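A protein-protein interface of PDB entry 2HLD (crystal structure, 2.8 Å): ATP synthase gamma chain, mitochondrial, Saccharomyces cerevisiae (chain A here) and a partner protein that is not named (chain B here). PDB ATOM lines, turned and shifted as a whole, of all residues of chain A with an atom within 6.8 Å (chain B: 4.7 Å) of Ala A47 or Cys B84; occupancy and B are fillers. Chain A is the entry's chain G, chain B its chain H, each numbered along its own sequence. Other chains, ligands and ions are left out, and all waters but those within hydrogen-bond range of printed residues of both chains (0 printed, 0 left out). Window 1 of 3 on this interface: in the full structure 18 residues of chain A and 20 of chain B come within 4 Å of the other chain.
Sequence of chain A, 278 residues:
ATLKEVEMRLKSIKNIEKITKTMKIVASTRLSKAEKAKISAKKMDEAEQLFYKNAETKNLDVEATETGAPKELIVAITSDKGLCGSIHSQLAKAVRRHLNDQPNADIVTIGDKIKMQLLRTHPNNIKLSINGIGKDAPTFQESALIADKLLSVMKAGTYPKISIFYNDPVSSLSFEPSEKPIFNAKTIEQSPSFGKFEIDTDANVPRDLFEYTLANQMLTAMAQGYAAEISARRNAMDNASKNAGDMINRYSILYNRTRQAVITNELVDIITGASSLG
CA of Met A44 touches CB of Ala B15, at 3.8 Å. Met A44 touches Thr B86 (CE to CB, 3.7 Å). Glu A46 touches Gln B13 (O to OE1, 3.9 Å). OE1 of Gln B13 touches CA of Ala A47 (3.9 Å). OG1 of Thr B86 touches OE1 of Glu A48, at 3.7 Å. CD2 of Leu A50 touches OE1 of Gln B13, 3.3 Å away. Leu A50 touches Gln B78 (CD2 to CG, 3.8 Å). Cys B84 touches Leu A50.
Of chain B, only Gln B13 (3.9 Å) and Cys B84 (3.8 Å) come within 4 Å of Ala A47. Of chain A, only Ala A47 and Leu A50 come within 4 Å of Cys B84. Printed residues of chain A within 4 Å of Gln B78: Leu A50 and Phe A51. Of the printed residues of chain B, Leu A50 touches Gln B13 (3.3 Å), Gln B78 (3.8 Å) and Cys B84 (3.8 Å). Printed residues of chain B within 4 Å of Met A44: Ala B15 (3.8 Å) and Thr B86 (3.7 Å).
Of the 10 printed residues of chain A, 6 touch a printed residue of chain B. Hydrophobic or aromatic side chains of chain A that line the printed part of chain B: Met A44 and Leu A50. Of the 11 printed residues of chain B, 5 touch a printed residue of chain A. Hydrophobic or aromatic side chains of chain B within 4 Å of the printed part of chain A: Ala B15.
N of Gln B13 lies within hydrogen-bond range of O of Leu B83. The backbone NH (N) of Ala B15 lies within hydrogen-bond range of the backbone carbonyl oxygen (O) of Val B85, at 3.2 Å. The side-chain amide oxygen of Gln B13 is in hydrogen-bond range of the side-chain sulfur of Cys B84, 3.4 Å away. N of Val B85 sits at hydrogen-bond distance from O of Gln B13. The backbone NH (N) of Cys B84 is in hydrogen-bond range of the backbone carbonyl oxygen (O) of Thr B76 (2.7 Å). N of Thr B86 is in hydrogen-bond range of O of Phe B74 (3.0 Å).
The side-chain sulfur (SG) of Cys B84 sits at hydrogen-bond distance from the backbone carbonyl oxygen (O) of Ala A47. The side-chain amide nitrogen (NE2) of Gln B78 lies close to the backbone NH (N) of Phe A51 (3.4 Å).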
ATOM      1  N   LYS A  42     -26.257 -24.126 -21.268  1.00  0.00           N
ATOM      2  CA  LYS A  42     -26.534 -22.895 -20.510  1.00  0.00           C
ATOM      3  C   LYS A  42     -26.019 -22.921 -19.064  1.00  0.00           C
ATOM      4  O   LYS A  42     -25.851 -21.863 -18.449  1.00  0.00           O
ATOM      5  CB  LYS A  42     -28.025 -22.535 -20.545  1.00  0.00           C
ATOM      6  CG  LYS A  42     -28.384 -21.406 -21.517  1.00  0.00           C
ATOM      7  CD  LYS A  42     -29.891 -21.179 -21.538  1.00  0.00           C
ATOM      8  CE  LYS A  42     -30.235 -19.706 -21.663  1.00  0.00           C
ATOM      9  NZ  LYS A  42     -31.596 -19.424 -21.131  1.00  0.00           N
ATOM     10  N   LYS A  43     -25.802 -24.120 -18.517  1.00  0.00           N
ATOM     11  CA  LYS A  43     -25.168 -24.270 -17.199  1.00  0.00           C
ATOM     12  C   LYS A  43     -23.674 -23.987 -17.314  1.00  0.00           C
ATOM     13  O   LYS A  43     -23.099 -23.301 -16.462  1.00  0.00           O
ATOM     14  CB  LYS A  43     -25.391 -25.673 -16.609  1.00  0.00           C
ATOM     15  CG  LYS A  43     -26.804 -25.959 -16.061  1.00  0.00           C
ATOM     16  CD  LYS A  43     -27.097 -25.254 -14.730  1.00  0.00           C
ATOM     17  CE  LYS A  43     -28.489 -25.603 -14.220  1.00  0.00           C
ATOM     18  NZ  LYS A  43     -28.947 -24.626 -13.195  1.00  0.00           N
ATOM     19  N   MET A  44     -23.059 -24.516 -18.373  1.00  0.00           N
ATOM     20  CA  MET A  44     -21.655 -24.244 -18.683  1.00  0.00           C
ATOM     21  C   MET A  44     -21.450 -22.783 -19.114  1.00  0.00           C
ATOM     22  O   MET A  44     -20.333 -22.264 -19.103  1.00  0.00           O
ATOM     23  CB  MET A  44     -21.169 -25.186 -19.776  1.00  0.00           C
ATOM     24  CG  MET A  44     -19.676 -25.359 -19.822  1.00  0.00           C
ATOM     25  SD  MET A  44     -19.281 -26.009 -21.425  1.00  0.00           S
ATOM     26  CE  MET A  44     -17.630 -26.677 -21.249  1.00  0.00           C
ATOM     27  N   ASP A  45     -22.547 -22.136 -19.495  1.00  0.00           N
ATOM     28  CA  ASP A  45     -22.550 -20.731 -19.870  1.00  0.00           C
ATOM     29  C   ASP A  45     -22.489 -19.829 -18.648  1.00  0.00           C
ATOM     30  O   ASP A  45     -21.970 -18.721 -18.719  1.00  0.00           O
ATOM     31  CB  ASP A  45     -23.810 -20.410 -20.659  1.00  0.00           C
ATOM     32  CG  ASP A  45     -23.659 -19.182 -21.509  1.00  0.00           C
ATOM     33  OD1 ASP A  45     -22.611 -19.051 -22.180  1.00  0.00           O
ATOM     34  OD2 ASP A  45     -24.541 -18.300 -21.577  1.00  0.00           O
ATOM     35  N   GLU A  46     -23.036 -20.297 -17.530  1.00  0.00           N
ATOM     36  CA  GLU A  46     -22.963 -19.544 -16.278  1.00  0.00           C
ATOM     37  C   GLU A  46     -21.736 -19.922 -15.436  1.00  0.00           C
ATOM     38  O   GLU A  46     -21.329 -19.149 -14.568  1.00  0.00           O
ATOM     39  CB  GLU A  46     -24.275 -19.636 -15.482  1.00  0.00           C
ATOM     40  CG  GLU A  46     -25.364 -18.705 -16.022  1.00  0.00           C
ATOM     41  CD  GLU A  46     -26.484 -18.409 -15.028  1.00  0.00           C
ATOM     42  OE1 GLU A  46     -26.910 -19.331 -14.291  1.00  0.00           O
ATOM     43  OE2 GLU A  46     -26.953 -17.248 -14.991  1.00  0.00           O
ATOM     44  N   ALA A  47     -21.155 -21.097 -15.699  1.00  0.00           N
ATOM     45  CA  ALA A  47     -19.883 -21.494 -15.087  1.00  0.00           C
ATOM     46  C   ALA A  47     -18.714 -20.755 -15.753  1.00  0.00           C
ATOM     47  O   ALA A  47     -17.837 -20.226 -15.077  1.00  0.00           O
ATOM     48  CB  ALA A  47     -19.693 -23.004 -15.179  1.00  0.00           C
ATOM     49  N   GLU A  48     -18.735 -20.714 -17.083  1.00  0.00           N
ATOM     50  CA  GLU A  48     -17.716 -20.051 -17.899  1.00  0.00           C
ATOM     51  C   GLU A  48     -17.764 -18.520 -17.793  1.00  0.00           C
ATOM     52  O   GLU A  48     -16.729 -17.859 -17.764  1.00  0.00           O
ATOM     53  CB  GLU A  48     -17.886 -20.492 -19.363  1.00  0.00           C
ATOM     54  CG  GLU A  48     -16.951 -19.851 -20.383  1.00  0.00           C
ATOM     55  CD  GLU A  48     -15.572 -20.498 -20.426  1.00  0.00           C
ATOM     56  OE1 GLU A  48     -15.271 -21.369 -19.566  1.00  0.00           O
ATOM     57  OE2 GLU A  48     -14.785 -20.126 -21.329  1.00  0.00           O
ATOM     58  N   GLN A  49     -18.974 -17.976 -17.722  1.00  0.00           N
ATOM     59  CA  GLN A  49     -19.222 -16.534 -17.842  1.00  0.00           C
ATOM     60  C   GLN A  49     -19.186 -15.789 -16.500  1.00  0.00           C
ATOM     61  O   GLN A  49     -19.139 -14.556 -16.471  1.00  0.00           O
ATOM     62  CB  GLN A  49     -20.596 -16.330 -18.475  1.00  0.00           C
ATOM     63  CG  GLN A  49     -20.680 -15.345 -19.621  1.00  0.00           C
ATOM     64  CD  GLN A  49     -22.105 -15.232 -20.169  1.00  0.00           C
ATOM     65  OE1 GLN A  49     -23.057 -15.765 -19.574  1.00  0.00           O
ATOM     66  NE2 GLN A  49     -22.253 -14.539 -21.302  1.00  0.00           N
ATOM     67  N   LEU A  50     -19.242 -16.548 -15.403  1.00  0.00           N
ATOM     68  CA  LEU A  50     -19.187 -16.016 -14.039  1.00  0.00           C
ATOM     69  C   LEU A  50     -17.860 -15.285 -13.836  1.00  0.00           C
ATOM     70  O   LEU A  50     -17.832 -14.176 -13.294  1.00  0.00           O
ATOM     71  CB  LEU A  50     -19.348 -17.160 -13.027  1.00  0.00           C
ATOM     72  CG  LEU A  50     -19.789 -16.996 -11.563  1.00  0.00           C
ATOM     73  CD1 LEU A  50     -21.070 -16.162 -11.407  1.00  0.00           C
ATOM     74  CD2 LEU A  50     -19.965 -18.372 -10.917  1.00  0.00           C
ATOM     75  N   PHE A  51     -16.766 -15.896 -14.295  1.00  0.00           N
ATOM     76  CA  PHE A  51     -15.485 -15.208 -14.314  1.00  0.00           C
ATOM     77  C   PHE A  51     -15.610 -13.777 -14.855  1.00  0.00           C
ATOM     78  O   PHE A  51     -15.328 -12.827 -14.133  1.00  0.00           O
ATOM     79  CB  PHE A  51     -14.432 -15.982 -15.098  1.00  0.00           C
ATOM     80  CG  PHE A  51     -13.290 -15.135 -15.529  1.00  0.00           C
ATOM     81  CD1 PHE A  51     -12.341 -14.703 -14.602  1.00  0.00           C
ATOM     82  CD2 PHE A  51     -13.176 -14.727 -16.841  1.00  0.00           C
ATOM     83  CE1 PHE A  51     -11.278 -13.887 -14.986  1.00  0.00           C
ATOM     84  CE2 PHE A  51     -12.121 -13.915 -17.239  1.00  0.00           C
ATOM     85  CZ  PHE A  51     -11.165 -13.496 -16.311  1.00  0.00           C
ATOM     86  N   GLN B  13     -19.209 -25.699  -9.263  1.00  0.00           N
ATOM     87  CA  GLN B  13     -19.832 -25.768 -10.573  1.00  0.00           C
ATOM     88  C   GLN B  13     -18.902 -26.558 -11.487  1.00  0.00           C
ATOM     89  O   GLN B  13     -17.859 -26.053 -11.912  1.00  0.00           O
ATOM     90  CB  GLN B  13     -20.113 -24.365 -11.125  1.00  0.00           C
ATOM     91  CG  GLN B  13     -21.230 -23.616 -10.391  1.00  0.00           C
ATOM     92  CD  GLN B  13     -21.821 -22.468 -11.206  1.00  0.00           C
ATOM     93  OE1 GLN B  13     -21.159 -21.454 -11.442  1.00  0.00           O
ATOM     94  NE2 GLN B  13     -23.071 -22.624 -11.627  1.00  0.00           N
ATOM     95  N   ALA B  15     -19.195 -28.472 -15.034  1.00  0.00           N
ATOM     96  CA  ALA B  15     -20.061 -28.564 -16.222  1.00  0.00           C
ATOM     97  C   ALA B  15     -19.303 -28.956 -17.486  1.00  0.00           C
ATOM     98  O   ALA B  15     -18.276 -28.371 -17.809  1.00  0.00           O
ATOM     99  CB  ALA B  15     -20.831 -27.250 -16.443  1.00  0.00           C
ATOM    100  N   PHE B  74     -10.746 -25.398 -18.060  1.00  0.00           N
ATOM    101  CA  PHE B  74     -10.514 -24.223 -17.214  1.00  0.00           C
ATOM    102  C   PHE B  74     -11.153 -24.306 -15.818  1.00  0.00           C
ATOM    103  O   PHE B  74     -12.333 -24.653 -15.689  1.00  0.00           O
ATOM    104  CB  PHE B  74     -11.030 -22.948 -17.921  1.00  0.00           C
ATOM    105  CG  PHE B  74      -9.998 -22.254 -18.772  1.00  0.00           C
ATOM    106  CD1 PHE B  74      -9.797 -22.625 -20.098  1.00  0.00           C
ATOM    107  CD2 PHE B  74      -9.234 -21.220 -18.251  1.00  0.00           C
ATOM    108  CE1 PHE B  74      -8.839 -21.997 -20.884  1.00  0.00           C
ATOM    109  CE2 PHE B  74      -8.274 -20.576 -19.040  1.00  0.00           C
ATOM    110  CZ  PHE B  74      -8.078 -20.974 -20.360  1.00  0.00           C
ATOM    111  N   ALA B  75     -10.372 -23.972 -14.783  1.00  0.00           N
ATOM    112  CA  ALA B  75     -10.913 -23.733 -13.443  1.00  0.00           C
ATOM    113  C   ALA B  75     -10.860 -22.236 -13.067  1.00  0.00           C
ATOM    114  O   ALA B  75      -9.923 -21.526 -13.455  1.00  0.00           O
ATOM    115  CB  ALA B  75     -10.203 -24.590 -12.401  1.00  0.00           C
ATOM    116  N   THR B  76     -11.893 -21.768 -12.355  1.00  0.00           N
ATOM    117  CA  THR B  76     -11.909 -20.436 -11.732  1.00  0.00           C
ATOM    118  C   THR B  76     -12.537 -20.490 -10.331  1.00  0.00           C
ATOM    119  O   THR B  76     -13.663 -20.964 -10.171  1.00  0.00           O
ATOM    120  CB  THR B  76     -12.662 -19.343 -12.600  1.00  0.00           C
ATOM    121  OG1 THR B  76     -14.035 -19.709 -12.783  1.00  0.00           O
ATOM    122  CG2 THR B  76     -12.128 -19.239 -14.029  1.00  0.00           C
ATOM    123  N   GLN B  78     -14.151 -18.158  -7.783  1.00  0.00           N
ATOM    124  CA  GLN B  78     -14.740 -16.835  -7.670  1.00  0.00           C
ATOM    125  C   GLN B  78     -14.570 -16.267  -6.254  1.00  0.00           C
ATOM    126  O   GLN B  78     -14.336 -17.021  -5.301  1.00  0.00           O
ATOM    127  CB  GLN B  78     -16.224 -16.875  -8.060  1.00  0.00           C
ATOM    128  CG  GLN B  78     -16.528 -17.587  -9.390  1.00  0.00           C
ATOM    129  CD  GLN B  78     -15.813 -16.983 -10.599  1.00  0.00           C
ATOM    130  OE1 GLN B  78     -15.336 -15.845 -10.548  1.00  0.00           O
ATOM    131  NE2 GLN B  78     -15.748 -17.744 -11.690  1.00  0.00           N
ATOM    132  N   GLN B  82     -16.812 -20.030  -4.593  1.00  0.00           N
ATOM    133  CA  GLN B  82     -17.275 -21.122  -5.456  1.00  0.00           C
ATOM    134  C   GLN B  82     -16.218 -21.458  -6.509  1.00  0.00           C
ATOM    135  O   GLN B  82     -15.631 -20.551  -7.102  1.00  0.00           O
ATOM    136  CB  GLN B  82     -18.602 -20.763  -6.132  1.00  0.00           C
ATOM    137  N   LEU B  83     -15.959 -22.751  -6.718  1.00  0.00           N
ATOM    138  CA  LEU B  83     -15.045 -23.188  -7.788  1.00  0.00           C
ATOM    139  C   LEU B  83     -15.811 -23.526  -9.067  1.00  0.00           C
ATOM    140  O   LEU B  83     -16.907 -24.094  -9.011  1.00  0.00           O
ATOM    141  CB  LEU B  83     -14.173 -24.373  -7.349  1.00  0.00           C
ATOM    142  CG  LEU B  83     -13.291 -25.070  -8.403  1.00  0.00           C
ATOM    143  CD1 LEU B  83     -12.215 -24.148  -8.984  1.00  0.00           C
ATOM    144  CD2 LEU B  83     -12.660 -26.337  -7.837  1.00  0.00           C
ATOM    145  N   CYS B  84     -15.223 -23.160 -10.209  1.00  0.00           N
ATOM    146  CA  CYS B  84     -15.803 -23.411 -11.532  1.00  0.00           C
ATOM    147  C   CYS B  84     -14.867 -24.188 -12.449  1.00  0.00           C
ATOM    148  O   CYS B  84     -13.837 -23.689 -12.881  1.00  0.00           O
ATOM    149  CB  CYS B  84     -16.237 -22.106 -12.190  1.00  0.00           C
ATOM    150  SG  CYS B  84     -17.769 -21.442 -11.504  1.00  0.00           S
ATOM    151  N   VAL B  85     -15.256 -25.423 -12.730  1.00  0.00           N
ATOM    152  CA  VAL B  85     -14.528 -26.316 -13.615  1.00  0.00           C
ATOM    153  C   VAL B  85     -15.366 -26.521 -14.885  1.00  0.00           C
ATOM    154  O   VAL B  85     -16.582 -26.692 -14.807  1.00  0.00           O
ATOM    155  CB  VAL B  85     -14.297 -27.684 -12.923  1.00  0.00           C
ATOM    156  CG1 VAL B  85     -13.419 -28.591 -13.774  1.00  0.00           C
ATOM    157  CG2 VAL B  85     -13.693 -27.493 -11.532  1.00  0.00           C
ATOM    158  N   THR B  86     -14.718 -26.462 -16.047  1.00  0.00           N
ATOM    159  CA  THR B  86     -15.333 -26.897 -17.306  1.00  0.00           C
ATOM    160  C   THR B  86     -14.343 -27.691 -18.149  1.00  0.00           C
ATOM    161  O   THR B  86     -13.134 -27.440 -18.116  1.00  0.00           O
ATOM    162  CB  THR B  86     -15.929 -25.723 -18.154  1.00  0.00           C
ATOM    163  OG1 THR B  86     -14.882 -24.957 -18.763  1.00  0.00           O
ATOM    164  CG2 THR B  86     -16.720 -24.713 -17.303  1.00  0.00           C
